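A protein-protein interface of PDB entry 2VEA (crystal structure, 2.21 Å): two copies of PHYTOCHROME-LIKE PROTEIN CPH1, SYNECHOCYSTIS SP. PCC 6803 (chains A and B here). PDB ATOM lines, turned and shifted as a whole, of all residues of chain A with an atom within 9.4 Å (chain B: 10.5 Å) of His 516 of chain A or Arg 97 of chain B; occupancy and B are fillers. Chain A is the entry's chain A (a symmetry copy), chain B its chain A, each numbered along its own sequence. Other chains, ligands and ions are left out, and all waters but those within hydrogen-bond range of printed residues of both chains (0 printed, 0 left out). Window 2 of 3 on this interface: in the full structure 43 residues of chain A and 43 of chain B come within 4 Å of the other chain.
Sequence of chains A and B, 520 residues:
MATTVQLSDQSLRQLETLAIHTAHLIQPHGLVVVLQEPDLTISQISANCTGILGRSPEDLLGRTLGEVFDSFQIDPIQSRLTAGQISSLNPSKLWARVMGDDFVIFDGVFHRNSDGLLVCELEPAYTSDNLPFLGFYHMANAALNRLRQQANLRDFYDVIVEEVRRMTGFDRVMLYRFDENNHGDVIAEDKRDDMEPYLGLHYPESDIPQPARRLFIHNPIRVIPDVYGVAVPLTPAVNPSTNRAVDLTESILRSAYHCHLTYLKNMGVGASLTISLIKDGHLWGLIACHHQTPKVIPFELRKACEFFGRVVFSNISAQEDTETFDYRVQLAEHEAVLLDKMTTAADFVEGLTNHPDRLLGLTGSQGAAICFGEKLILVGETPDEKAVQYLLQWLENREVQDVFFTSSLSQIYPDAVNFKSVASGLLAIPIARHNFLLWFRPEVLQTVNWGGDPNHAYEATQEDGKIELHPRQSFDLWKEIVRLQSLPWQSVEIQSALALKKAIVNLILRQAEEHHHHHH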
ATOM      1  N   ILE A 508      27.354 -34.191   1.194  1.00  0.00           N
ATOM      2  CA  ILE A 508      27.041 -34.129  -0.239  1.00  0.00           C
ATOM      3  C   ILE A 508      27.621 -32.851  -0.852  1.00  0.00           C
ATOM      4  O   ILE A 508      28.214 -32.886  -1.936  1.00  0.00           O
ATOM      5  CB  ILE A 508      25.511 -34.185  -0.528  1.00  0.00           C
ATOM      6  CG1 ILE A 508      24.945 -35.591  -0.287  1.00  0.00           C
ATOM      7  CG2 ILE A 508      25.216 -33.773  -1.968  1.00  0.00           C
ATOM      8  CD1 ILE A 508      24.367 -35.797   1.091  1.00  0.00           C
ATOM      9  N   LEU A 509      27.456 -31.730  -0.149  1.00  0.00           N
ATOM     10  CA  LEU A 509      28.041 -30.452  -0.571  1.00  0.00           C
ATOM     11  C   LEU A 509      29.574 -30.474  -0.568  1.00  0.00           C
ATOM     12  O   LEU A 509      30.202 -29.875  -1.444  1.00  0.00           O
ATOM     13  CB  LEU A 509      27.534 -29.297   0.306  1.00  0.00           C
ATOM     14  CG  LEU A 509      26.223 -28.623  -0.118  1.00  0.00           C
ATOM     15  CD1 LEU A 509      26.406 -27.860  -1.425  1.00  0.00           C
ATOM     16  CD2 LEU A 509      25.105 -29.635  -0.241  1.00  0.00           C
ATOM     17  N   ARG A 510      30.174 -31.153   0.408  1.00  0.00           N
ATOM     18  CA  ARG A 510      31.638 -31.277   0.464  1.00  0.00           C
ATOM     19  C   ARG A 510      32.153 -32.025  -0.767  1.00  0.00           C
ATOM     20  O   ARG A 510      33.109 -31.584  -1.402  1.00  0.00           O
ATOM     21  CB  ARG A 510      32.093 -31.981   1.748  1.00  0.00           C
ATOM     22  CG  ARG A 510      33.542 -31.719   2.114  1.00  0.00           C
ATOM     23  N   GLN A 511      31.504 -33.143  -1.101  1.00  0.00           N
ATOM     24  CA  GLN A 511      31.790 -33.884  -2.336  1.00  0.00           C
ATOM     25  C   GLN A 511      31.617 -33.003  -3.569  1.00  0.00           C
ATOM     26  O   GLN A 511      32.505 -32.933  -4.421  1.00  0.00           O
ATOM     27  CB  GLN A 511      30.852 -35.085  -2.488  1.00  0.00           C
ATOM     28  CG  GLN A 511      31.062 -36.217  -1.498  1.00  0.00           C
ATOM     29  CD  GLN A 511      30.162 -37.415  -1.796  1.00  0.00           C
ATOM     30  OE1 GLN A 511      30.334 -38.099  -2.813  1.00  0.00           O
ATOM     31  NE2 GLN A 511      29.200 -37.675  -0.903  1.00  0.00           N
ATOM     32  N   ALA A 512      30.464 -32.343  -3.652  1.00  0.00           N
ATOM     33  CA  ALA A 512      30.116 -31.506  -4.800  1.00  0.00           C
ATOM     34  C   ALA A 512      31.225 -30.521  -5.164  1.00  0.00           C
ATOM     35  O   ALA A 512      31.591 -30.401  -6.337  1.00  0.00           O
ATOM     36  CB  ALA A 512      28.821 -30.760  -4.527  1.00  0.00           C
ATOM     37  N   GLU A 513      31.756 -29.825  -4.158  1.00  0.00           N
ATOM     38  CA  GLU A 513      32.824 -28.844  -4.379  1.00  0.00           C
ATOM     39  C   GLU A 513      34.213 -29.482  -4.453  1.00  0.00           C
ATOM     40  O   GLU A 513      35.158 -28.850  -4.926  1.00  0.00           O
ATOM     41  CB  GLU A 513      32.782 -27.732  -3.318  1.00  0.00           C
ATOM     42  CG  GLU A 513      33.347 -28.082  -1.948  1.00  0.00           C
ATOM     43  CD  GLU A 513      33.109 -26.968  -0.935  1.00  0.00           C
ATOM     44  OE1 GLU A 513      34.081 -26.264  -0.580  1.00  0.00           O
ATOM     45  OE2 GLU A 513      31.947 -26.787  -0.507  1.00  0.00           O
ATOM     46  N   GLU A 514      34.338 -30.725  -3.991  1.00  0.00           N
ATOM     47  CA  GLU A 514      35.563 -31.502  -4.196  1.00  0.00           C
ATOM     48  C   GLU A 514      35.736 -31.860  -5.678  1.00  0.00           C
ATOM     49  O   GLU A 514      36.863 -32.010  -6.156  1.00  0.00           O
ATOM     50  CB  GLU A 514      35.554 -32.773  -3.342  1.00  0.00           C
ATOM     51  N   HIS A 515      34.616 -31.987  -6.396  1.00  0.00           N
ATOM     52  CA  HIS A 515      34.630 -32.228  -7.844  1.00  0.00           C
ATOM     53  C   HIS A 515      34.575 -30.937  -8.681  1.00  0.00           C
ATOM     54  O   HIS A 515      34.481 -31.003  -9.907  1.00  0.00           O
ATOM     55  CB  HIS A 515      33.477 -33.160  -8.239  1.00  0.00           C
ATOM     56  CG  HIS A 515      33.669 -34.576  -7.796  1.00  0.00           C
ATOM     57  ND1 HIS A 515      34.555 -35.435  -8.411  1.00  0.00           N
ATOM     58  CD2 HIS A 515      33.089 -35.286  -6.799  1.00  0.00           C
ATOM     59  CE1 HIS A 515      34.514 -36.612  -7.811  1.00  0.00           C
ATOM     60  NE2 HIS A 515      33.632 -36.548  -6.830  1.00  0.00           N
ATOM     61  N   HIS A 516      34.640 -29.778  -8.023  1.00  0.00           N
ATOM     62  CA  HIS A 516      34.632 -28.486  -8.712  1.00  0.00           C
ATOM     63  C   HIS A 516      36.035 -27.894  -8.781  1.00  0.00           C
ATOM     64  O   HIS A 516      36.781 -27.935  -7.804  1.00  0.00           O
ATOM     65  CB  HIS A 516      33.704 -27.497  -8.007  1.00  0.00           C
ATOM     66  CG  HIS A 516      33.639 -26.159  -8.677  1.00  0.00           C
ATOM     67  ND1 HIS A 516      34.622 -25.203  -8.527  1.00  0.00           N
ATOM     68  CD2 HIS A 516      32.721 -25.626  -9.516  1.00  0.00           C
ATOM     69  CE1 HIS A 516      34.308 -24.136  -9.240  1.00  0.00           C
ATOM     70  NE2 HIS A 516      33.158 -24.365  -9.847  1.00  0.00           N
ATOM     71  N   HIS A 517      36.366 -27.317  -9.936  1.00  0.00           N
ATOM     72  CA  HIS A 517      37.711 -26.834 -10.239  1.00  0.00           C
ATOM     73  C   HIS A 517      37.635 -25.463 -10.916  1.00  0.00           C
ATOM     74  O   HIS A 517      36.629 -25.137 -11.543  1.00  0.00           O
ATOM     75  CB  HIS A 517      38.421 -27.842 -11.145  1.00  0.00           C
ATOM     76  CG  HIS A 517      38.286 -29.261 -10.686  1.00  0.00           C
ATOM     77  ND1 HIS A 517      39.210 -29.872  -9.866  1.00  0.00           N
ATOM     78  CD2 HIS A 517      37.324 -30.185 -10.919  1.00  0.00           C
ATOM     79  CE1 HIS A 517      38.826 -31.112  -9.620  1.00  0.00           C
ATOM     80  NE2 HIS A 517      37.685 -31.327 -10.248  1.00  0.00           N
ATOM     81  N   HIS A 518      38.707 -24.679 -10.807  1.00  0.00           N
ATOM     82  CA  HIS A 518      38.668 -23.257 -11.172  1.00  0.00           C
ATOM     83  C   HIS A 518      39.375 -22.861 -12.485  1.00  0.00           C
ATOM     84  O   HIS A 518      40.532 -23.202 -12.718  1.00  0.00           O
ATOM     85  CB  HIS A 518      39.250 -22.408 -10.033  1.00  0.00           C
ATOM     86  CG  HIS A 518      38.475 -22.487  -8.754  1.00  0.00           C
ATOM     87  ND1 HIS A 518      37.122 -22.233  -8.683  1.00  0.00           N
ATOM     88  CD2 HIS A 518      38.869 -22.772  -7.490  1.00  0.00           C
ATOM     89  CE1 HIS A 518      36.712 -22.371  -7.434  1.00  0.00           C
ATOM     90  NE2 HIS A 518      37.754 -22.697  -6.689  1.00  0.00           N
ATOM     91  N   HIS A 519      38.614 -22.182 -13.342  1.00  0.00           N
ATOM     92  CA  HIS A 519      39.092 -21.170 -14.318  1.00  0.00           C
ATOM     93  C   HIS A 519      39.539 -21.614 -15.733  1.00  0.00           C
ATOM     94  O   HIS A 519      38.731 -21.553 -16.658  1.00  0.00           O
ATOM     95  CB  HIS A 519      40.041 -20.128 -13.656  1.00  0.00           C
ATOM     96  CG  HIS A 519      41.505 -20.422 -13.780  1.00  0.00           C
ATOM     97  ND1 HIS A 519      42.266 -19.970 -14.836  1.00  0.00           N
ATOM     98  CD2 HIS A 519      42.359 -21.074 -12.956  1.00  0.00           C
ATOM     99  CE1 HIS A 519      43.518 -20.358 -14.675  1.00  0.00           C
ATOM    100  NE2 HIS A 519      43.601 -21.028 -13.541  1.00  0.00           N
ATOM    101  N   ILE B  52      30.838 -11.574  -5.552  1.00  0.00           N
ATOM    102  CA  ILE B  52      30.805 -12.964  -5.075  1.00  0.00           C
ATOM    103  C   ILE B  52      29.878 -13.892  -5.869  1.00  0.00           C
ATOM    104  O   ILE B  52      30.171 -15.083  -5.993  1.00  0.00           O
ATOM    105  CB  ILE B  52      30.462 -13.043  -3.566  1.00  0.00           C
ATOM    106  CG1 ILE B  52      29.052 -12.518  -3.277  1.00  0.00           C
ATOM    107  CG2 ILE B  52      31.498 -12.268  -2.757  1.00  0.00           C
ATOM    108  CD1 ILE B  52      28.764 -12.372  -1.798  1.00  0.00           C
ATOM    109  N   LEU B  53      28.772 -13.360  -6.389  1.00  0.00           N
ATOM    110  CA  LEU B  53      27.898 -14.122  -7.292  1.00  0.00           C
ATOM    111  C   LEU B  53      28.332 -13.980  -8.754  1.00  0.00           C
ATOM    112  O   LEU B  53      28.354 -14.963  -9.492  1.00  0.00           O
ATOM    113  CB  LEU B  53      26.435 -13.686  -7.150  1.00  0.00           C
ATOM    114  CG  LEU B  53      25.763 -13.915  -5.797  1.00  0.00           C
ATOM    115  CD1 LEU B  53      24.347 -13.374  -5.831  1.00  0.00           C
ATOM    116  CD2 LEU B  53      25.758 -15.390  -5.429  1.00  0.00           C
ATOM    117  N   GLY B  54      28.668 -12.757  -9.165  1.00  0.00           N
ATOM    118  CA  GLY B  54      29.033 -12.471 -10.555  1.00  0.00           C
ATOM    119  C   GLY B  54      27.891 -11.844 -11.339  1.00  0.00           C
ATOM    120  O   GLY B  54      28.120 -11.133 -12.319  1.00  0.00           O
ATOM    121  N   ARG B  55      26.662 -12.116 -10.906  1.00  0.00           N
ATOM    122  CA  ARG B  55      25.461 -11.524 -11.498  1.00  0.00           C
ATOM    123  C   ARG B  55      24.995 -10.387 -10.590  1.00  0.00           C
ATOM    124  O   ARG B  55      24.748 -10.595  -9.401  1.00  0.00           O
ATOM    125  CB  ARG B  55      24.354 -12.579 -11.695  1.00  0.00           C
ATOM    126  CG  ARG B  55      24.318 -13.690 -10.640  1.00  0.00           C
ATOM    127  CD  ARG B  55      23.052 -14.538 -10.712  1.00  0.00           C
ATOM    128  NE  ARG B  55      23.058 -15.497 -11.821  1.00  0.00           N
ATOM    129  CZ  ARG B  55      22.300 -15.422 -12.918  1.00  0.00           C
ATOM    130  NH1 ARG B  55      21.441 -14.421 -13.103  1.00  0.00           N
ATOM    131  NH2 ARG B  55      22.404 -16.367 -13.848  1.00  0.00           N
ATOM    132  N   ASP B  59      21.471  -8.600 -13.872  1.00  0.00           N
ATOM    133  CA  ASP B  59      21.015  -9.979 -14.069  1.00  0.00           C
ATOM    134  C   ASP B  59      20.016 -10.417 -13.001  1.00  0.00           C
ATOM    135  O   ASP B  59      19.044 -11.109 -13.306  1.00  0.00           O
ATOM    136  CB  ASP B  59      22.207 -10.944 -14.084  1.00  0.00           C
ATOM    137  CG  ASP B  59      23.097 -10.766 -15.304  1.00  0.00           C
ATOM    138  OD1 ASP B  59      22.882  -9.810 -16.081  1.00  0.00           O
ATOM    139  OD2 ASP B  59      24.020 -11.588 -15.484  1.00  0.00           O
ATOM    140  N   LEU B  60      20.259 -10.009 -11.756  1.00  0.00           N
ATOM    141  CA  LEU B  60      19.388 -10.370 -10.636  1.00  0.00           C
ATOM    142  C   LEU B  60      18.177  -9.433 -10.533  1.00  0.00           C
ATOM    143  O   LEU B  60      17.426  -9.290 -11.502  1.00  0.00           O
ATOM    144  CB  LEU B  60      20.182 -10.416  -9.322  1.00  0.00           C
ATOM    145  CG  LEU B  60      21.216 -11.531  -9.202  1.00  0.00           C
ATOM    146  CD1 LEU B  60      22.043 -11.345  -7.942  1.00  0.00           C
ATOM    147  CD2 LEU B  60      20.519 -12.876  -9.191  1.00  0.00           C
ATOM    148  N   GLU B  67      15.713 -19.801  -9.107  1.00  0.00           N
ATOM    149  CA  GLU B  67      16.971 -20.176  -9.752  1.00  0.00           C
ATOM    150  C   GLU B  67      17.874 -18.981 -10.063  1.00  0.00           C
ATOM    151  O   GLU B  67      18.169 -18.666 -11.216  1.00  0.00           O
ATOM    152  CB  GLU B  67      16.735 -21.064 -10.990  1.00  0.00           C
ATOM    153  CG  GLU B  67      16.568 -22.562 -10.666  1.00  0.00           C
ATOM    154  CD  GLU B  67      17.665 -23.107  -9.748  1.00  0.00           C
ATOM    155  OE1 GLU B  67      18.863 -22.980 -10.088  1.00  0.00           O
ATOM    156  OE2 GLU B  67      17.320 -23.659  -8.682  1.00  0.00           O
ATOM    157  N   VAL B  68      18.253 -18.293  -8.994  1.00  0.00           N
ATOM    158  CA  VAL B  68      19.575 -17.689  -8.891  1.00  0.00           C
ATOM    159  C   VAL B  68      20.393 -18.653  -8.033  1.00  0.00           C
ATOM    160  O   VAL B  68      21.570 -18.897  -8.310  1.00  0.00           O
ATOM    161  CB  VAL B  68      19.562 -16.277  -8.261  1.00  0.00           C
ATOM    162  CG1 VAL B  68      18.675 -16.232  -7.029  1.00  0.00           C
ATOM    163  CG2 VAL B  68      20.982 -15.829  -7.916  1.00  0.00           C
ATOM    164  N   PHE B  69      19.742 -19.213  -7.008  1.00  0.00           N
ATOM    165  CA  PHE B  69      20.347 -20.190  -6.110  1.00  0.00           C
ATOM    166  C   PHE B  69      19.700 -21.566  -6.235  1.00  0.00           C
ATOM    167  O   PHE B  69      18.597 -21.706  -6.759  1.00  0.00           O
ATOM    168  CB  PHE B  69      20.211 -19.722  -4.664  1.00  0.00           C
ATOM    169  CG  PHE B  69      20.848 -18.396  -4.396  1.00  0.00           C
ATOM    170  CD1 PHE B  69      22.206 -18.306  -4.135  1.00  0.00           C
ATOM    171  CD2 PHE B  69      20.090 -17.237  -4.393  1.00  0.00           C
ATOM    172  CE1 PHE B  69      22.799 -17.079  -3.885  1.00  0.00           C
ATOM    173  CE2 PHE B  69      20.671 -16.007  -4.144  1.00  0.00           C
ATOM    174  CZ  PHE B  69      22.028 -15.925  -3.892  1.00  0.00           C
ATOM    175  N   ASP B  70      20.413 -22.574  -5.736  1.00  0.00           N
ATOM    176  CA  ASP B  70      19.924 -23.949  -5.652  1.00  0.00           C
ATOM    177  C   ASP B  70      19.875 -24.360  -4.184  1.00  0.00           C
ATOM    178  O   ASP B  70      20.560 -23.768  -3.356  1.00  0.00           O
ATOM    179  CB  ASP B  70      20.860 -24.882  -6.420  1.00  0.00           C
ATOM    180  CG  ASP B  70      20.601 -24.875  -7.911  1.00  0.00           C
ATOM    181  OD1 ASP B  70      19.534 -25.375  -8.318  1.00  0.00           O
ATOM    182  OD2 ASP B  70      21.464 -24.386  -8.675  1.00  0.00           O
ATOM    183  N   SER B  71      19.061 -25.363  -3.866  1.00  0.00           N
ATOM    184  CA  SER B  71      18.959 -25.877  -2.500  1.00  0.00           C
ATOM    185  C   SER B  71      18.244 -27.228  -2.458  1.00  0.00           C
ATOM    186  O   SER B  71      17.895 -27.783  -3.497  1.00  0.00           O
ATOM    187  CB  SER B  71      18.227 -24.873  -1.598  1.00  0.00           C
ATOM    188  OG  SER B  71      16.831 -24.890  -1.822  1.00  0.00           O
ATOM    189  N   LEU B  94      22.042 -22.748   0.656  1.00  0.00           N
ATOM    190  CA  LEU B  94      21.797 -22.230  -0.680  1.00  0.00           C
ATOM    191  C   LEU B  94      23.127 -22.120  -1.404  1.00  0.00           C
ATOM    192  O   LEU B  94      24.107 -21.654  -0.834  1.00  0.00           O
ATOM    193  CB  LEU B  94      21.115 -20.858  -0.629  1.00  0.00           C
ATOM    194  CG  LEU B  94      19.625 -20.862  -0.272  1.00  0.00           C
ATOM    195  CD1 LEU B  94      19.455 -20.909   1.239  1.00  0.00           C
ATOM    196  CD2 LEU B  94      18.927 -19.651  -0.844  1.00  0.00           C
ATOM    197  N   TRP B  95      23.167 -22.550  -2.660  1.00  0.00           N
ATOM    198  CA  TRP B  95      24.393 -22.461  -3.439  1.00  0.00           C
ATOM    199  C   TRP B  95      24.116 -22.014  -4.859  1.00  0.00           C
ATOM    200  O   TRP B  95      23.006 -22.182  -5.366  1.00  0.00           O
ATOM    201  CB  TRP B  95      25.122 -23.803  -3.446  1.00  0.00           C
ATOM    202  CG  TRP B  95      24.355 -24.926  -4.070  1.00  0.00           C
ATOM    203  CD1 TRP B  95      24.301 -25.235  -5.392  1.00  0.00           C
ATOM    204  CD2 TRP B  95      23.554 -25.904  -3.396  1.00  0.00           C
ATOM    205  NE1 TRP B  95      23.515 -26.340  -5.589  1.00  0.00           N
ATOM    206  CE2 TRP B  95      23.043 -26.771  -4.380  1.00  0.00           C
ATOM    207  CE3 TRP B  95      23.219 -26.129  -2.055  1.00  0.00           C
ATOM    208  CZ2 TRP B  95      22.210 -27.848  -4.072  1.00  0.00           C
ATOM    209  CZ3 TRP B  95      22.391 -27.201  -1.747  1.00  0.00           C
ATOM    210  CH2 TRP B  95      21.896 -28.047  -2.755  1.00  0.00           C
ATOM    211  N   ALA B  96      25.138 -21.440  -5.487  1.00  0.00           N
ATOM    212  CA  ALA B  96      25.072 -21.049  -6.893  1.00  0.00           C
ATOM    213  C   ALA B  96      26.365 -21.419  -7.617  1.00  0.00           C
ATOM    214  O   ALA B  96      27.445 -21.445  -7.017  1.00  0.00           O
ATOM    215  CB  ALA B  96      24.805 -19.556  -7.017  1.00  0.00           C
ATOM    216  N   ARG B  97      26.232 -21.721  -8.906  1.00  0.00           N
ATOM    217  CA  ARG B  97      27.368 -21.939  -9.791  1.00  0.00           C
ATOM    218  C   ARG B  97      27.431 -20.778 -10.773  1.00  0.00           C
ATOM    219  O   ARG B  97      26.487 -20.561 -11.536  1.00  0.00           O
ATOM    220  CB  ARG B  97      27.228 -23.273 -10.541  1.00  0.00           C
ATOM    221  CG  ARG B  97      28.182 -24.363 -10.058  1.00  0.00           C
ATOM    222  CD  ARG B  97      27.596 -25.767 -10.176  1.00  0.00           C
ATOM    223  NE  ARG B  97      28.395 -26.742  -9.426  1.00  0.00           N
ATOM    224  CZ  ARG B  97      29.458 -27.398  -9.898  1.00  0.00           C
ATOM    225  NH1 ARG B  97      29.891 -27.213 -11.145  1.00  0.00           N
ATOM    226  NH2 ARG B  97      30.103 -28.257  -9.109  1.00  0.00           N
ATOM    227  N   VAL B  98      28.527 -20.023 -10.732  1.00  0.00           N
ATOM    228  CA  VAL B  98      28.756 -18.933 -11.685  1.00  0.00           C
ATOM    229  C   VAL B  98      30.225 -18.898 -12.112  1.00  0.00           C
ATOM    230  O   VAL B  98      31.091 -18.492 -11.337  1.00  0.00           O
ATOM    231  CB  VAL B  98      28.372 -17.560 -11.092  1.00  0.00           C
ATOM    232  CG1 VAL B  98      28.477 -16.478 -12.166  1.00  0.00           C
ATOM    233  CG2 VAL B  98      26.967 -17.595 -10.496  1.00  0.00           C
ATOM    234  N   MET B  99      30.497 -19.324 -13.344  1.00  0.00           N
ATOM    235  CA  MET B  99      31.867 -19.384 -13.860  1.00  0.00           C
ATOM    236  C   MET B  99      32.384 -17.987 -14.190  1.00  0.00           C
ATOM    237  O   MET B  99      33.072 -17.364 -13.383  1.00  0.00           O
ATOM    238  CB  MET B  99      31.944 -20.278 -15.102  1.00  0.00           C
ATOM    239  CG  MET B  99      31.682 -21.761 -14.840  1.00  0.00           C
ATOM    240  SD  MET B  99      29.943 -22.169 -14.556  1.00  0.00           S
ATOM    241  CE  MET B  99      29.862 -22.230 -12.768  1.00  0.00           C
ATOM    242  N   ASP B 102      32.384 -20.960 -10.953  1.00  0.00           N
ATOM    243  CA  ASP B 102      32.792 -20.821  -9.561  1.00  0.00           C
ATOM    244  C   ASP B 102      31.626 -21.155  -8.623  1.00  0.00           C
ATOM    245  O   ASP B 102      30.502 -20.678  -8.815  1.00  0.00           O
ATOM    246  CB  ASP B 102      33.310 -19.404  -9.292  1.00  0.00           C
ATOM    247  CG  ASP B 102      34.602 -19.399  -8.498  1.00  0.00           C
ATOM    248  OD1 ASP B 102      34.605 -18.900  -7.353  1.00  0.00           O
ATOM    249  OD2 ASP B 102      35.615 -19.903  -9.025  1.00  0.00           O
ATOM    250  N   PHE B 103      31.916 -21.962  -7.604  1.00  0.00           N
ATOM    251  CA  PHE B 103      30.894 -22.600  -6.782  1.00  0.00           C
ATOM    252  C   PHE B 103      30.883 -22.017  -5.372  1.00  0.00           C
ATOM    253  O   PHE B 103      31.812 -22.248  -4.593  1.00  0.00           O
ATOM    254  CB  PHE B 103      31.162 -24.110  -6.744  1.00  0.00           C
ATOM    255  CG  PHE B 103      30.106 -24.909  -6.032  1.00  0.00           C
ATOM    256  CD1 PHE B 103      28.777 -24.835  -6.421  1.00  0.00           C
ATOM    257  CD2 PHE B 103      30.447 -25.762  -4.991  1.00  0.00           C
ATOM    258  CE1 PHE B 103      27.801 -25.575  -5.773  1.00  0.00           C
ATOM    259  CE2 PHE B 103      29.472 -26.510  -4.337  1.00  0.00           C
ATOM    260  CZ  PHE B 103      28.147 -26.415  -4.729  1.00  0.00           C
ATOM    261  N   VAL B 104      29.830 -21.260  -5.058  1.00  0.00           N
ATOM    262  CA  VAL B 104      29.671 -20.630  -3.743  1.00  0.00           C
ATOM    263  C   VAL B 104      28.545 -21.297  -2.958  1.00  0.00           C
ATOM    264  O   VAL B 104      27.480 -21.572  -3.508  1.00  0.00           O
ATOM    265  CB  VAL B 104      29.352 -19.128  -3.865  1.00  0.00           C
ATOM    266  CG1 VAL B 104      29.435 -18.460  -2.496  1.00  0.00           C
ATOM    267  CG2 VAL B 104      30.299 -18.453  -4.849  1.00  0.00           C
ATOM    268  N   ILE B 105      28.793 -21.539  -1.672  1.00  0.00           N
ATOM    269  CA  ILE B 105      27.844 -22.214  -0.789  1.00  0.00           C
ATOM    270  C   ILE B 105      27.517 -21.315   0.399  1.00  0.00           C
ATOM    271  O   ILE B 105      28.407 -20.937   1.168  1.00  0.00           O
ATOM    272  CB  ILE B 105      28.413 -23.549  -0.255  1.00  0.00           C
ATOM    273  CG1 ILE B 105      28.862 -24.450  -1.409  1.00  0.00           C
ATOM    274  CG2 ILE B 105      27.385 -24.271   0.606  1.00  0.00           C
ATOM    275  CD1 ILE B 105      30.248 -24.133  -1.920  1.00  0.00           C
ATOM    276  N   PHE B 106      26.238 -20.979   0.542  1.00  0.00           N
ATOM    277  CA  PHE B 106      25.767 -20.130   1.626  1.00  0.00           C
ATOM    278  C   PHE B 106      24.920 -20.911   2.620  1.00  0.00           C
ATOM    279  O   PHE B 106      24.399 -21.978   2.303  1.00  0.00           O
ATOM    280  CB  PHE B 106      24.935 -18.978   1.071  1.00  0.00           C
ATOM    281  CG  PHE B 106      25.698 -18.063   0.159  1.00  0.00           C
ATOM    282  CD1 PHE B 106      26.591 -17.135   0.679  1.00  0.00           C
ATOM    283  CD2 PHE B 106      25.514 -18.118  -1.216  1.00  0.00           C
ATOM    284  CE1 PHE B 106      27.294 -16.281  -0.153  1.00  0.00           C
ATOM    285  CE2 PHE B 106      26.215 -17.269  -2.060  1.00  0.00           C
ATOM    286  CZ  PHE B 106      27.106 -16.346  -1.527  1.00  0.00           C
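OD2 of Asp 102 of chain B lies within hydrogen-bond range of ND1 of His 518 of chain A (2.8 Å).
The backbone carbonyl oxygen of Trp 95 of chain B is in hydrogen-bond range of the backbone NH of Asp 70 of chain B (2.6 Å).
Leu 509 of chain A touches Trp 95 of chain B (CD1 to CE3, 3.7 Å).
Arg 97 of chain B touches Ala 512 of chain A.
Glu 513 of chain A touches Phe 103 of chain B (CB to CD2, 3.5 Å).
Glu 513 of chain A touches Ile 105 of chain B (OE2 to CD1, 3.5 Å).
His 516 of chain A touches Arg 97 of chain B (CD2 to NH1, 3.6 Å).
His 516 of chain A touches Asp 102 of chain B.
Phe 103 of chain B touches His 516 of chain A.
Of the printed residues of chain B, Ala 512 of chain A touches Arg 97 (3.8 Å).
Of the printed residues of chain B, Glu 513 of chain A touches Phe 103 and Ile 105.
No residue of chain B comes within 4 Å of Glu 514 of chain A.
No residue of chain B comes within 4 Å of His 517 of chain A.
Printed residues of chain A within 4 Å of Trp 95 of chain B: Leu 509.
Ala 96 of chain B touches none of the printed residues of chain A.
Arg 97 of chain B touches just these residues of chain A: Ala 512 (3.8 Å) and His 516 (3.6 Å).
No residue of chain A comes within 4 Å of Val 98 of chain B.
Printed residues of chain A within 4 Å of Asp 102 of chain B: His 516 (3.6 Å) and His 518 (2.8 Å).
Of the printed residues of chain A, Ile 105 of chain B touches Glu 513 (3.5 Å).
The nearest residue of chain B that does not touch His 516 of chain A is Met 99 of chain B (4.9 Å).
Of the 12 printed residues of chain A, 5 touch a printed residue of chain B.
Hydrophobic or aromatic side chains of chain A within 4 Å of the printed part of chain B: Leu 509, His 516 and His 518.
Printed residues of chain B that touch a printed residue of chain A: Trp 95, Arg 97, Asp 102, Phe 103 and Ile 105.
Among the printed residues, 8 pairs touch across the chains.
Among the printed residues, no Asp or Glu carboxylate lies within 4 Å of a Lys or Arg side-chain nitrogen of the other chain.
No position is printed for both chains.
Of the 8 pairs that touch across the chains among the printed residues, none has its exchanged pair printed and touching as well.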
